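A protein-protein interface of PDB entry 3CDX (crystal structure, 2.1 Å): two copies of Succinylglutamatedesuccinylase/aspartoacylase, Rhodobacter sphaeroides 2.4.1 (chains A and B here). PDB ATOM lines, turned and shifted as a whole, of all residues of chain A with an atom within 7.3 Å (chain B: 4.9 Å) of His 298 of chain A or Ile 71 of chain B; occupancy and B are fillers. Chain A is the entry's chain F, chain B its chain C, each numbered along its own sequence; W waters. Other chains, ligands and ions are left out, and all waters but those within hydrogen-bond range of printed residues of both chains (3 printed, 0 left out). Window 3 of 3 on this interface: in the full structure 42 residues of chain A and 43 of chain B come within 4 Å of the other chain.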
ATOM      1  N   THR A 275     -21.253   6.397  29.689  1.00  0.00           N
ATOM      2  CA  THR A 275     -21.502   6.775  28.329  1.00  0.00           C
ATOM      3  C   THR A 275     -20.172   7.245  27.695  1.00  0.00           C
ATOM      4  O   THR A 275     -19.385   8.019  28.308  1.00  0.00           O
ATOM      5  CB  THR A 275     -22.619   7.851  28.292  1.00  0.00           C
ATOM      6  OG1 THR A 275     -23.845   7.258  28.770  1.00  0.00           O
ATOM      7  CG2 THR A 275     -22.827   8.419  26.832  1.00  0.00           C
ATOM      8  N   GLY A 276     -19.871   6.736  26.506  1.00  0.00           N
ATOM      9  CA  GLY A 276     -18.620   7.133  25.862  1.00  0.00           C
ATOM     10  C   GLY A 276     -18.444   6.436  24.543  1.00  0.00           C
ATOM     11  O   GLY A 276     -19.408   5.889  23.983  1.00  0.00           O
ATOM     12  N   LEU A 277     -17.220   6.451  24.042  1.00  0.00           N
ATOM     13  CA  LEU A 277     -16.923   5.829  22.757  1.00  0.00           C
ATOM     14  C   LEU A 277     -16.159   4.540  23.015  1.00  0.00           C
ATOM     15  O   LEU A 277     -14.992   4.562  23.463  1.00  0.00           O
ATOM     16  CB  LEU A 277     -16.137   6.804  21.863  1.00  0.00           C
ATOM     17  CG  LEU A 277     -15.560   6.283  20.543  1.00  0.00           C
ATOM     18  CD1 LEU A 277     -16.614   5.517  19.707  1.00  0.00           C
ATOM     19  CD2 LEU A 277     -14.944   7.441  19.750  1.00  0.00           C
ATOM     20  N   PHE A 278     -16.829   3.421  22.772  1.00  0.00           N
ATOM     21  CA  PHE A 278     -16.292   2.118  23.071  1.00  0.00           C
ATOM     22  C   PHE A 278     -15.492   1.498  21.901  1.00  0.00           C
ATOM     23  O   PHE A 278     -15.999   1.309  20.768  1.00  0.00           O
ATOM     24  CB  PHE A 278     -17.377   1.159  23.598  1.00  0.00           C
ATOM     25  CG  PHE A 278     -16.859  -0.223  23.913  1.00  0.00           C
ATOM     26  CD1 PHE A 278     -16.104  -0.447  25.062  1.00  0.00           C
ATOM     27  CD2 PHE A 278     -17.104  -1.293  23.059  1.00  0.00           C
ATOM     28  CE1 PHE A 278     -15.575  -1.729  25.351  1.00  0.00           C
ATOM     29  CE2 PHE A 278     -16.585  -2.598  23.339  1.00  0.00           C
ATOM     30  CZ  PHE A 278     -15.821  -2.812  24.473  1.00  0.00           C
ATOM     31  N   GLU A 279     -14.225   1.224  22.195  1.00  0.00           N
ATOM     32  CA  GLU A 279     -13.323   0.506  21.298  1.00  0.00           C
ATOM     33  C   GLU A 279     -13.160  -0.899  21.853  1.00  0.00           C
ATOM     34  O   GLU A 279     -12.585  -1.057  22.962  1.00  0.00           O
ATOM     35  CB  GLU A 279     -11.959   1.197  21.292  1.00  0.00           C
ATOM     36  CG  GLU A 279     -10.910   0.490  20.384  1.00  0.00           C
ATOM     37  CD  GLU A 279      -9.488   0.949  20.667  1.00  0.00           C
ATOM     38  OE1 GLU A 279      -9.260   1.953  21.406  1.00  0.00           O
ATOM     39  OE2 GLU A 279      -8.611   0.244  20.171  1.00  0.00           O
ATOM     40  N   PRO A 280     -13.668  -1.903  21.117  1.00  0.00           N
ATOM     41  CA  PRO A 280     -13.587  -3.312  21.428  1.00  0.00           C
ATOM     42  C   PRO A 280     -12.217  -3.870  21.124  1.00  0.00           C
ATOM     43  O   PRO A 280     -11.489  -3.291  20.313  1.00  0.00           O
ATOM     44  CB  PRO A 280     -14.610  -3.947  20.445  1.00  0.00           C
ATOM     45  CG  PRO A 280     -14.632  -2.993  19.269  1.00  0.00           C
ATOM     46  CD  PRO A 280     -14.425  -1.652  19.866  1.00  0.00           C
ATOM     47  N   GLY A 295     -12.164  -3.965  25.998  1.00  0.00           N
ATOM     48  CA  GLY A 295     -12.042  -2.716  25.244  1.00  0.00           C
ATOM     49  C   GLY A 295     -11.953  -1.550  26.207  1.00  0.00           C
ATOM     50  O   GLY A 295     -11.639  -1.746  27.398  1.00  0.00           O
ATOM     51  N   TRP A 296     -12.186  -0.334  25.686  1.00  0.00           N
ATOM     52  CA  TRP A 296     -12.019   0.894  26.435  1.00  0.00           C
ATOM     53  C   TRP A 296     -13.152   1.820  26.058  1.00  0.00           C
ATOM     54  O   TRP A 296     -13.516   1.937  24.875  1.00  0.00           O
ATOM     55  CB  TRP A 296     -10.690   1.599  26.124  1.00  0.00           C
ATOM     56  CG  TRP A 296      -9.454   0.765  26.374  1.00  0.00           C
ATOM     57  CD1 TRP A 296      -8.663   0.744  27.508  1.00  0.00           C
ATOM     58  CD2 TRP A 296      -8.873  -0.169  25.469  1.00  0.00           C
ATOM     59  NE1 TRP A 296      -7.645  -0.158  27.349  1.00  0.00           N
ATOM     60  CE2 TRP A 296      -7.752  -0.733  26.109  1.00  0.00           C
ATOM     61  CE3 TRP A 296      -9.199  -0.589  24.174  1.00  0.00           C
ATOM     62  CZ2 TRP A 296      -6.938  -1.692  25.487  1.00  0.00           C
ATOM     63  CZ3 TRP A 296      -8.395  -1.539  23.556  1.00  0.00           C
ATOM     64  CH2 TRP A 296      -7.267  -2.070  24.211  1.00  0.00           C
ATOM     65  N   ILE A 297     -13.730   2.457  27.067  1.00  0.00           N
ATOM     66  CA  ILE A 297     -14.630   3.557  26.831  1.00  0.00           C
ATOM     67  C   ILE A 297     -13.775   4.819  26.820  1.00  0.00           C
ATOM     68  O   ILE A 297     -13.164   5.184  27.818  1.00  0.00           O
ATOM     69  CB  ILE A 297     -15.726   3.626  27.904  1.00  0.00           C
ATOM     70  CG1 ILE A 297     -16.589   2.355  27.879  1.00  0.00           C
ATOM     71  CG2 ILE A 297     -16.615   4.850  27.678  1.00  0.00           C
ATOM     72  CD1 ILE A 297     -17.684   2.341  28.964  1.00  0.00           C
ATOM     73  N   HIS A 298     -13.709   5.452  25.664  1.00  0.00           N
ATOM     74  CA  HIS A 298     -13.037   6.707  25.465  1.00  0.00           C
ATOM     75  C   HIS A 298     -13.918   7.911  25.797  1.00  0.00           C
ATOM     76  O   HIS A 298     -15.117   7.923  25.447  1.00  0.00           O
ATOM     77  CB  HIS A 298     -12.621   6.801  23.981  1.00  0.00           C
ATOM     78  CG  HIS A 298     -11.581   5.796  23.562  1.00  0.00           C
ATOM     79  ND1 HIS A 298     -10.229   6.058  23.629  1.00  0.00           N
ATOM     80  CD2 HIS A 298     -11.696   4.553  23.036  1.00  0.00           C
ATOM     81  CE1 HIS A 298      -9.549   5.009  23.186  1.00  0.00           C
ATOM     82  NE2 HIS A 298     -10.417   4.085  22.798  1.00  0.00           N
ATOM     83  N   PHE A 299     -13.305   8.931  26.418  1.00  0.00           N
ATOM     84  CA  PHE A 299     -13.969  10.211  26.745  1.00  0.00           C
ATOM     85  C   PHE A 299     -13.453  11.374  25.891  1.00  0.00           C
ATOM     86  O   PHE A 299     -12.710  12.251  26.366  1.00  0.00           O
ATOM     87  CB  PHE A 299     -13.875  10.515  28.264  1.00  0.00           C
ATOM     88  CG  PHE A 299     -14.311   9.350  29.124  1.00  0.00           C
ATOM     89  CD1 PHE A 299     -15.668   9.053  29.271  1.00  0.00           C
ATOM     90  CD2 PHE A 299     -13.370   8.504  29.719  1.00  0.00           C
ATOM     91  CE1 PHE A 299     -16.071   7.938  30.046  1.00  0.00           C
ATOM     92  CE2 PHE A 299     -13.755   7.394  30.494  1.00  0.00           C
ATOM     93  CZ  PHE A 299     -15.106   7.116  30.672  1.00  0.00           C
ATOM     94  N   VAL A 300     -13.879  11.383  24.632  1.00  0.00           N
ATOM     95  CA  VAL A 300     -13.280  12.262  23.621  1.00  0.00           C
ATOM     96  C   VAL A 300     -13.643  13.724  23.830  1.00  0.00           C
ATOM     97  O   VAL A 300     -13.018  14.619  23.256  1.00  0.00           O
ATOM     98  CB  VAL A 300     -13.554  11.778  22.174  1.00  0.00           C
ATOM     99  CG1 VAL A 300     -12.997  10.370  21.965  1.00  0.00           C
ATOM    100  CG2 VAL A 300     -15.052  11.834  21.840  1.00  0.00           C
ATOM    101  N   GLU A 301     -14.597  13.956  24.725  1.00  0.00           N
ATOM    102  CA  GLU A 301     -15.028  15.294  25.129  1.00  0.00           C
ATOM    103  C   GLU A 301     -14.010  15.971  26.062  1.00  0.00           C
ATOM    104  O   GLU A 301     -14.062  17.187  26.270  1.00  0.00           O
ATOM    105  CB  GLU A 301     -16.403  15.185  25.841  1.00  0.00           C
ATOM    106  CG  GLU A 301     -16.389  14.368  27.141  1.00  0.00           C
ATOM    107  CD  GLU A 301     -16.762  12.872  26.976  1.00  0.00           C
ATOM    108  OE1 GLU A 301     -17.146  12.257  28.004  1.00  0.00           O
ATOM    109  OE2 GLU A 301     -16.693  12.316  25.847  1.00  0.00           O
ATOM    110  N   THR A 305      -8.002  13.037  29.815  1.00  0.00           N
ATOM    111  CA  THR A 305      -8.665  11.869  30.448  1.00  0.00           C
ATOM    112  C   THR A 305      -8.317  10.513  29.785  1.00  0.00           C
ATOM    113  O   THR A 305      -8.441  10.347  28.565  1.00  0.00           O
ATOM    114  CB  THR A 305     -10.185  12.096  30.574  1.00  0.00           C
ATOM    115  OG1 THR A 305     -10.412  13.383  31.159  1.00  0.00           O
ATOM    116  CG2 THR A 305     -10.829  11.048  31.442  1.00  0.00           C
ATOM    117  N   ALA A 306      -7.877   9.546  30.590  1.00  0.00           N
ATOM    118  CA  ALA A 306      -7.646   8.172  30.118  1.00  0.00           C
ATOM    119  C   ALA A 306      -8.947   7.428  29.839  1.00  0.00           C
ATOM    120  O   ALA A 306      -9.880   7.542  30.591  1.00  0.00           O
ATOM    121  CB  ALA A 306      -6.847   7.366  31.169  1.00  0.00           C
ATOM    122  N   PRO A 307      -8.968   6.580  28.808  1.00  0.00           N
ATOM    123  CA  PRO A 307     -10.172   5.787  28.580  1.00  0.00           C
ATOM    124  C   PRO A 307     -10.382   4.759  29.701  1.00  0.00           C
ATOM    125  O   PRO A 307      -9.428   4.374  30.396  1.00  0.00           O
ATOM    126  CB  PRO A 307      -9.901   5.114  27.221  1.00  0.00           C
ATOM    127  CG  PRO A 307      -8.466   5.108  27.082  1.00  0.00           C
ATOM    128  CD  PRO A 307      -7.905   6.267  27.836  1.00  0.00           C
ATOM    129  N   LEU A 308     -11.628   4.381  29.917  1.00  0.00           N
ATOM    130  CA  LEU A 308     -11.970   3.394  30.936  1.00  0.00           C
ATOM    131  C   LEU A 308     -11.859   1.964  30.391  1.00  0.00           C
ATOM    132  O   LEU A 308     -12.566   1.581  29.459  1.00  0.00           O
ATOM    133  CB  LEU A 308     -13.379   3.668  31.467  1.00  0.00           C
ATOM    134  CG  LEU A 308     -14.006   2.684  32.453  1.00  0.00           C
ATOM    135  CD1 LEU A 308     -13.189   2.710  33.745  1.00  0.00           C
ATOM    136  CD2 LEU A 308     -15.483   3.086  32.708  1.00  0.00           C
ATOM    137  N   GLY A 325     -20.685   2.845  17.976  1.00  0.00           N
ATOM    138  CA  GLY A 325     -19.433   3.276  18.621  1.00  0.00           C
ATOM    139  C   GLY A 325     -19.697   3.984  19.947  1.00  0.00           C
ATOM    140  O   GLY A 325     -19.021   3.747  20.943  1.00  0.00           O
ATOM    141  N   ARG A 326     -20.665   4.886  19.949  1.00  0.00           N
ATOM    142  CA  ARG A 326     -21.000   5.632  21.129  1.00  0.00           C
ATOM    143  C   ARG A 326     -21.989   4.812  21.948  1.00  0.00           C
ATOM    144  O   ARG A 326     -23.102   4.527  21.510  1.00  0.00           O
ATOM    145  CB  ARG A 326     -21.571   6.998  20.777  1.00  0.00           C
ATOM    146  CG  ARG A 326     -21.850   7.824  22.039  1.00  0.00           C
ATOM    147  CD  ARG A 326     -22.019   9.304  21.744  1.00  0.00           C
ATOM    148  NE  ARG A 326     -22.642  10.016  22.843  1.00  0.00           N
ATOM    149  CZ  ARG A 326     -21.986  10.539  23.872  1.00  0.00           C
ATOM    150  NH1 ARG A 326     -20.651  10.483  23.935  1.00  0.00           N
ATOM    151  NH2 ARG A 326     -22.668  11.181  24.810  1.00  0.00           N
ATOM    152  N   TYR B  67     -15.634   7.347  14.089  1.00  0.00           N
ATOM    153  CA  TYR B  67     -14.964   7.173  15.402  1.00  0.00           C
ATOM    154  C   TYR B  67     -13.438   7.068  15.362  1.00  0.00           C
ATOM    155  O   TYR B  67     -12.769   7.520  16.262  1.00  0.00           O
ATOM    156  CB  TYR B  67     -15.483   5.910  16.128  1.00  0.00           C
ATOM    157  CG  TYR B  67     -16.983   5.783  16.127  1.00  0.00           C
ATOM    158  CD1 TYR B  67     -17.786   6.783  16.702  1.00  0.00           C
ATOM    159  CD2 TYR B  67     -17.612   4.705  15.487  1.00  0.00           C
ATOM    160  CE1 TYR B  67     -19.190   6.691  16.662  1.00  0.00           C
ATOM    161  CE2 TYR B  67     -19.023   4.619  15.425  1.00  0.00           C
ATOM    162  CZ  TYR B  67     -19.775   5.612  16.020  1.00  0.00           C
ATOM    163  OH  TYR B  67     -21.122   5.523  16.001  1.00  0.00           O
ATOM    164  N   GLU B  68     -12.916   6.390  14.356  1.00  0.00           N
ATOM    165  CA  GLU B  68     -11.504   5.997  14.320  1.00  0.00           C
ATOM    166  C   GLU B  68     -10.537   7.185  14.512  1.00  0.00           C
ATOM    167  O   GLU B  68      -9.551   7.040  15.203  1.00  0.00           O
ATOM    168  CB  GLU B  68     -11.208   5.258  13.005  1.00  0.00           C
ATOM    169  CG  GLU B  68     -11.632   3.770  12.935  1.00  0.00           C
ATOM    170  CD  GLU B  68     -13.121   3.500  13.038  1.00  0.00           C
ATOM    171  OE1 GLU B  68     -13.949   4.448  13.017  1.00  0.00           O
ATOM    172  OE2 GLU B  68     -13.479   2.309  13.127  1.00  0.00           O
ATOM    173  N   GLY B  69     -10.809   8.341  13.891  1.00  0.00           N
ATOM    174  CA  GLY B  69     -10.037   9.555  14.137  1.00  0.00           C
ATOM    175  C   GLY B  69     -10.166  10.107  15.543  1.00  0.00           C
ATOM    176  O   GLY B  69      -9.206  10.623  16.139  1.00  0.00           O
ATOM    177  N   GLN B  70     -11.360  10.024  16.098  1.00  0.00           N
ATOM    178  CA  GLN B  70     -11.578  10.432  17.473  1.00  0.00           C
ATOM    179  C   GLN B  70     -10.711   9.611  18.442  1.00  0.00           C
ATOM    180  O   GLN B  70     -10.054  10.151  19.368  1.00  0.00           O
ATOM    181  CB  GLN B  70     -13.080  10.255  17.820  1.00  0.00           C
ATOM    182  CG  GLN B  70     -14.078  11.013  16.857  1.00  0.00           C
ATOM    183  CD  GLN B  70     -15.500  10.897  17.361  1.00  0.00           C
ATOM    184  OE1 GLN B  70     -15.758  11.033  18.563  1.00  0.00           O
ATOM    185  NE2 GLN B  70     -16.425  10.656  16.459  1.00  0.00           N
ATOM    186  N   ILE B  71     -10.742   8.300  18.252  1.00  0.00           N
ATOM    187  CA  ILE B  71      -9.924   7.388  19.038  1.00  0.00           C
ATOM    188  C   ILE B  71      -8.431   7.654  18.802  1.00  0.00           C
ATOM    189  O   ILE B  71      -7.668   7.901  19.764  1.00  0.00           O
ATOM    190  CB  ILE B  71     -10.255   5.907  18.718  1.00  0.00           C
ATOM    191  CG1 ILE B  71     -11.684   5.557  19.173  1.00  0.00           C
ATOM    192  CG2 ILE B  71      -9.247   4.960  19.401  1.00  0.00           C
ATOM    193  CD1 ILE B  71     -12.260   4.218  18.567  1.00  0.00           C
ATOM    194  N   ALA B  72      -8.000   7.595  17.545  1.00  0.00           N
ATOM    195  CA  ALA B  72      -6.554   7.618  17.253  1.00  0.00           C
ATOM    196  C   ALA B  72      -5.923   8.924  17.710  1.00  0.00           C
ATOM    197  O   ALA B  72      -4.932   8.919  18.453  1.00  0.00           O
ATOM    198  CB  ALA B  72      -6.334   7.381  15.768  1.00  0.00           C
ATOM    199  N   ILE B  73      -6.555  10.053  17.357  1.00  0.00           N
ATOM    200  CA  ILE B  73      -6.054  11.380  17.744  1.00  0.00           C
ATOM    201  C   ILE B  73      -6.116  11.684  19.245  1.00  0.00           C
ATOM    202  O   ILE B  73      -5.156  12.244  19.797  1.00  0.00           O
ATOM    203  CB  ILE B  73      -6.716  12.502  16.909  1.00  0.00           C
ATOM    204  CG1 ILE B  73      -6.400  12.262  15.442  1.00  0.00           C
ATOM    205  CG2 ILE B  73      -6.224  13.914  17.363  1.00  0.00           C
ATOM    206  CD1 ILE B  73      -7.284  13.054  14.524  1.00  0.00           C
ATOM    207  N   SER B  74      -7.214  11.294  19.913  1.00  0.00           N
ATOM    208  CA  SER B  74      -7.359  11.588  21.335  1.00  0.00           C
ATOM    209  C   SER B  74      -6.341  10.767  22.123  1.00  0.00           C
ATOM    210  O   SER B  74      -5.827  11.223  23.132  1.00  0.00           O
ATOM    211  CB  SER B  74      -8.802  11.365  21.863  1.00  0.00           C
ATOM    212  OG  SER B  74      -9.192   9.988  21.955  1.00  0.00           O
ATOM    213  N   ASP B  75      -6.084   9.554  21.650  1.00  0.00           N
ATOM    214  CA  ASP B  75      -5.061   8.681  22.231  1.00  0.00           C
ATOM    215  C   ASP B  75      -3.629   9.318  22.161  1.00  0.00           C
ATOM    216  O   ASP B  75      -2.915   9.419  23.176  1.00  0.00           O
ATOM    217  CB  ASP B  75      -5.098   7.290  21.538  1.00  0.00           C
ATOM    218  CG  ASP B  75      -3.985   6.371  22.025  1.00  0.00           C
ATOM    219  OD1 ASP B  75      -4.053   5.994  23.211  1.00  0.00           O
ATOM    220  OD2 ASP B  75      -3.045   6.064  21.234  1.00  0.00           O
ATOM    221  N   VAL B 221     -17.206   0.579  15.528  1.00  0.00           N
ATOM    222  CA  VAL B 221     -15.747   0.784  15.566  1.00  0.00           C
ATOM    223  C   VAL B 221     -14.996  -0.405  14.950  1.00  0.00           C
ATOM    224  O   VAL B 221     -15.218  -1.542  15.337  1.00  0.00           O
ATOM    225  CB  VAL B 221     -15.236   0.988  17.004  1.00  0.00           C
ATOM    226  CG1 VAL B 221     -13.745   1.108  17.017  1.00  0.00           C
ATOM    227  CG2 VAL B 221     -15.848   2.246  17.621  1.00  0.00           C
ATOM    228  N   VAL B 226      -8.939   1.259  13.537  1.00  0.00           N
ATOM    229  CA  VAL B 226      -8.220   1.896  14.632  1.00  0.00           C
ATOM    230  C   VAL B 226      -6.676   1.674  14.529  1.00  0.00           C
ATOM    231  O   VAL B 226      -5.901   2.638  14.641  1.00  0.00           O
ATOM    232  CB  VAL B 226      -8.718   1.426  16.002  1.00  0.00           C
ATOM    233  CG1 VAL B 226      -7.884   2.085  17.124  1.00  0.00           C
ATOM    234  CG2 VAL B 226     -10.237   1.725  16.189  1.00  0.00           C
ATOM    235  N   LYS B 230      -4.028   4.721  13.989  1.00  0.00           N
ATOM    236  CA  LYS B 230      -3.041   5.080  15.014  1.00  0.00           C
ATOM    237  C   LYS B 230      -1.614   5.048  14.454  1.00  0.00           C
ATOM    238  O   LYS B 230      -0.788   5.897  14.784  1.00  0.00           O
ATOM    239  CB  LYS B 230      -3.119   4.131  16.212  1.00  0.00           C
ATOM    240  CG  LYS B 230      -4.341   4.321  17.160  1.00  0.00           C
ATOM    241  CD  LYS B 230      -4.100   3.563  18.469  1.00  0.00           C
ATOM    242  CE  LYS B 230      -5.234   3.686  19.471  1.00  0.00           C
ATOM    243  NZ  LYS B 230      -4.877   2.972  20.758  1.00  0.00           N
HETATM  244  O   HOH W   1      -9.240   8.595  24.338  1.00  0.00           O
HETATM  245  O   HOH W   2      -7.176   2.706  22.593  1.00  0.00           O
HETATM  246  O   HOH W   3      -5.962   0.343  20.186  1.00  0.00           O
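The side-chain hydroxyl (OH) of Tyr 67 of chain B lies within hydrogen-bond range of the backbone NH (N) of Gly 325 of chain A, at 3.4 Å.
The backbone carbonyl oxygen of Ile 71 of chain B is in hydrogen-bond range of the side-chain hydroxyl of Ser 74 of chain B (3.4 Å).
O of Gln 70 of chain B lies within hydrogen-bond range of OG of Ser 74 of chain B, 2.7 Å away.
O of Glu 279 of chain A lies within hydrogen-bond range of N of Trp 296 of chain A, 2.8 Å away.
OE1 of Glu 279 of chain A is in hydrogen-bond range of NE2 of His 298 of chain A, 2.8 Å away.
The backbone carbonyl oxygen (O) of Leu 277 of chain A lies within hydrogen-bond range of the backbone NH (N) of His 298 of chain A (2.7 Å).
The backbone carbonyl oxygen (O) of Gly 325 of chain A sits at hydrogen-bond distance from the backbone NH (N) of Phe 278 of chain A (2.9 Å).
Tyr 67 of chain B touches Leu 277 of chain A.
Gln 70 of chain B touches Leu 277 of chain A.
Phe 278 of chain A touches Val 221 of chain B.
Glu 279 of chain A touches Ile 71 of chain B.
OE2 of Glu 279 of chain A touches CG1 of Val 226 of chain B, at 3.6 Å.
Val 221 of chain B touches Pro 280 of chain A (CB to CD, 3.98 Å).
CG2 of Ile 71 of chain B touches NE2 of His 298 of chain A, 3.7 Å away.
Val 300 of chain A touches Gln 70 of chain B (CG2 to OE1, 3.4 Å).
Val 300 of chain A touches Ser 74 of chain B (CG1 to OG, 3.8 Å).
CA of Gly 325 of chain A touches CG2 of Val 221 of chain B, at 3.9 Å.
Gly 276 of chain A touches none of the printed residues of chain B.
Printed residues of chain B within 4 Å of Leu 277 of chain A: Tyr 67 (3.5 Å), Gln 70 (3.9 Å), Ile 71 (3.8 Å) and Val 221 (3.95 Å).
Of the printed residues of chain B, Pro 280 of chain A touches Val 221 (3.98 Å).
Of chain B, only Ile 71 comes within 4 Å of His 298 of chain A.
Of the printed residues of chain B, Gly 325 of chain A touches Tyr 67 and Val 221.
Of the printed residues of chain A, Val 221 of chain B touches Leu 277 (3.95 Å), Phe 278 (3.3 Å), Pro 280 (3.98 Å) and Gly 325 (3.9 Å).
Lys 230 of chain B touches none of the printed residues of chain A.
The nearest residue of chain B that does not touch His 298 of chain A is Ser 74 of chain B (4.4 Å).
The nearest printed residue of chain A that does not touch Ile 71 of chain B is Val 300 of chain A (4.8 Å).
Hydrophobic or aromatic side chains of chain A within 4 Å of the printed part of chain B: Leu 277, Pro 280, His 298 and Val 300.
Hydrophobic or aromatic side chains of chain B that line the printed part of chain A: Tyr 67, Ile 71, Val 221 and Val 226.
Among the printed residues, no Asp or Glu carboxylate lies within 4 Å of a Lys or Arg side-chain nitrogen of the other chain.
No position is printed for both chains.
Of the 13 pairs that touch across the chains among the printed residues, none has its exchanged pair printed and touching as well.
Water W2 lies within hydrogen-bond range of OE1 of Glu 279 of chain A (2.5 Å) and NZ of Lys 230 of chain B (3.0 Å).
Water W3 bridges OE2 of Glu 279 of chain A (2.7 Å) and NZ of Lys 230 of chain B (2.9 Å).
Water W1 lies within hydrogen-bond range of OG of Ser 74 of chain B (2.8 Å) and ND1 of His 298 of chain A (2.8 Å).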
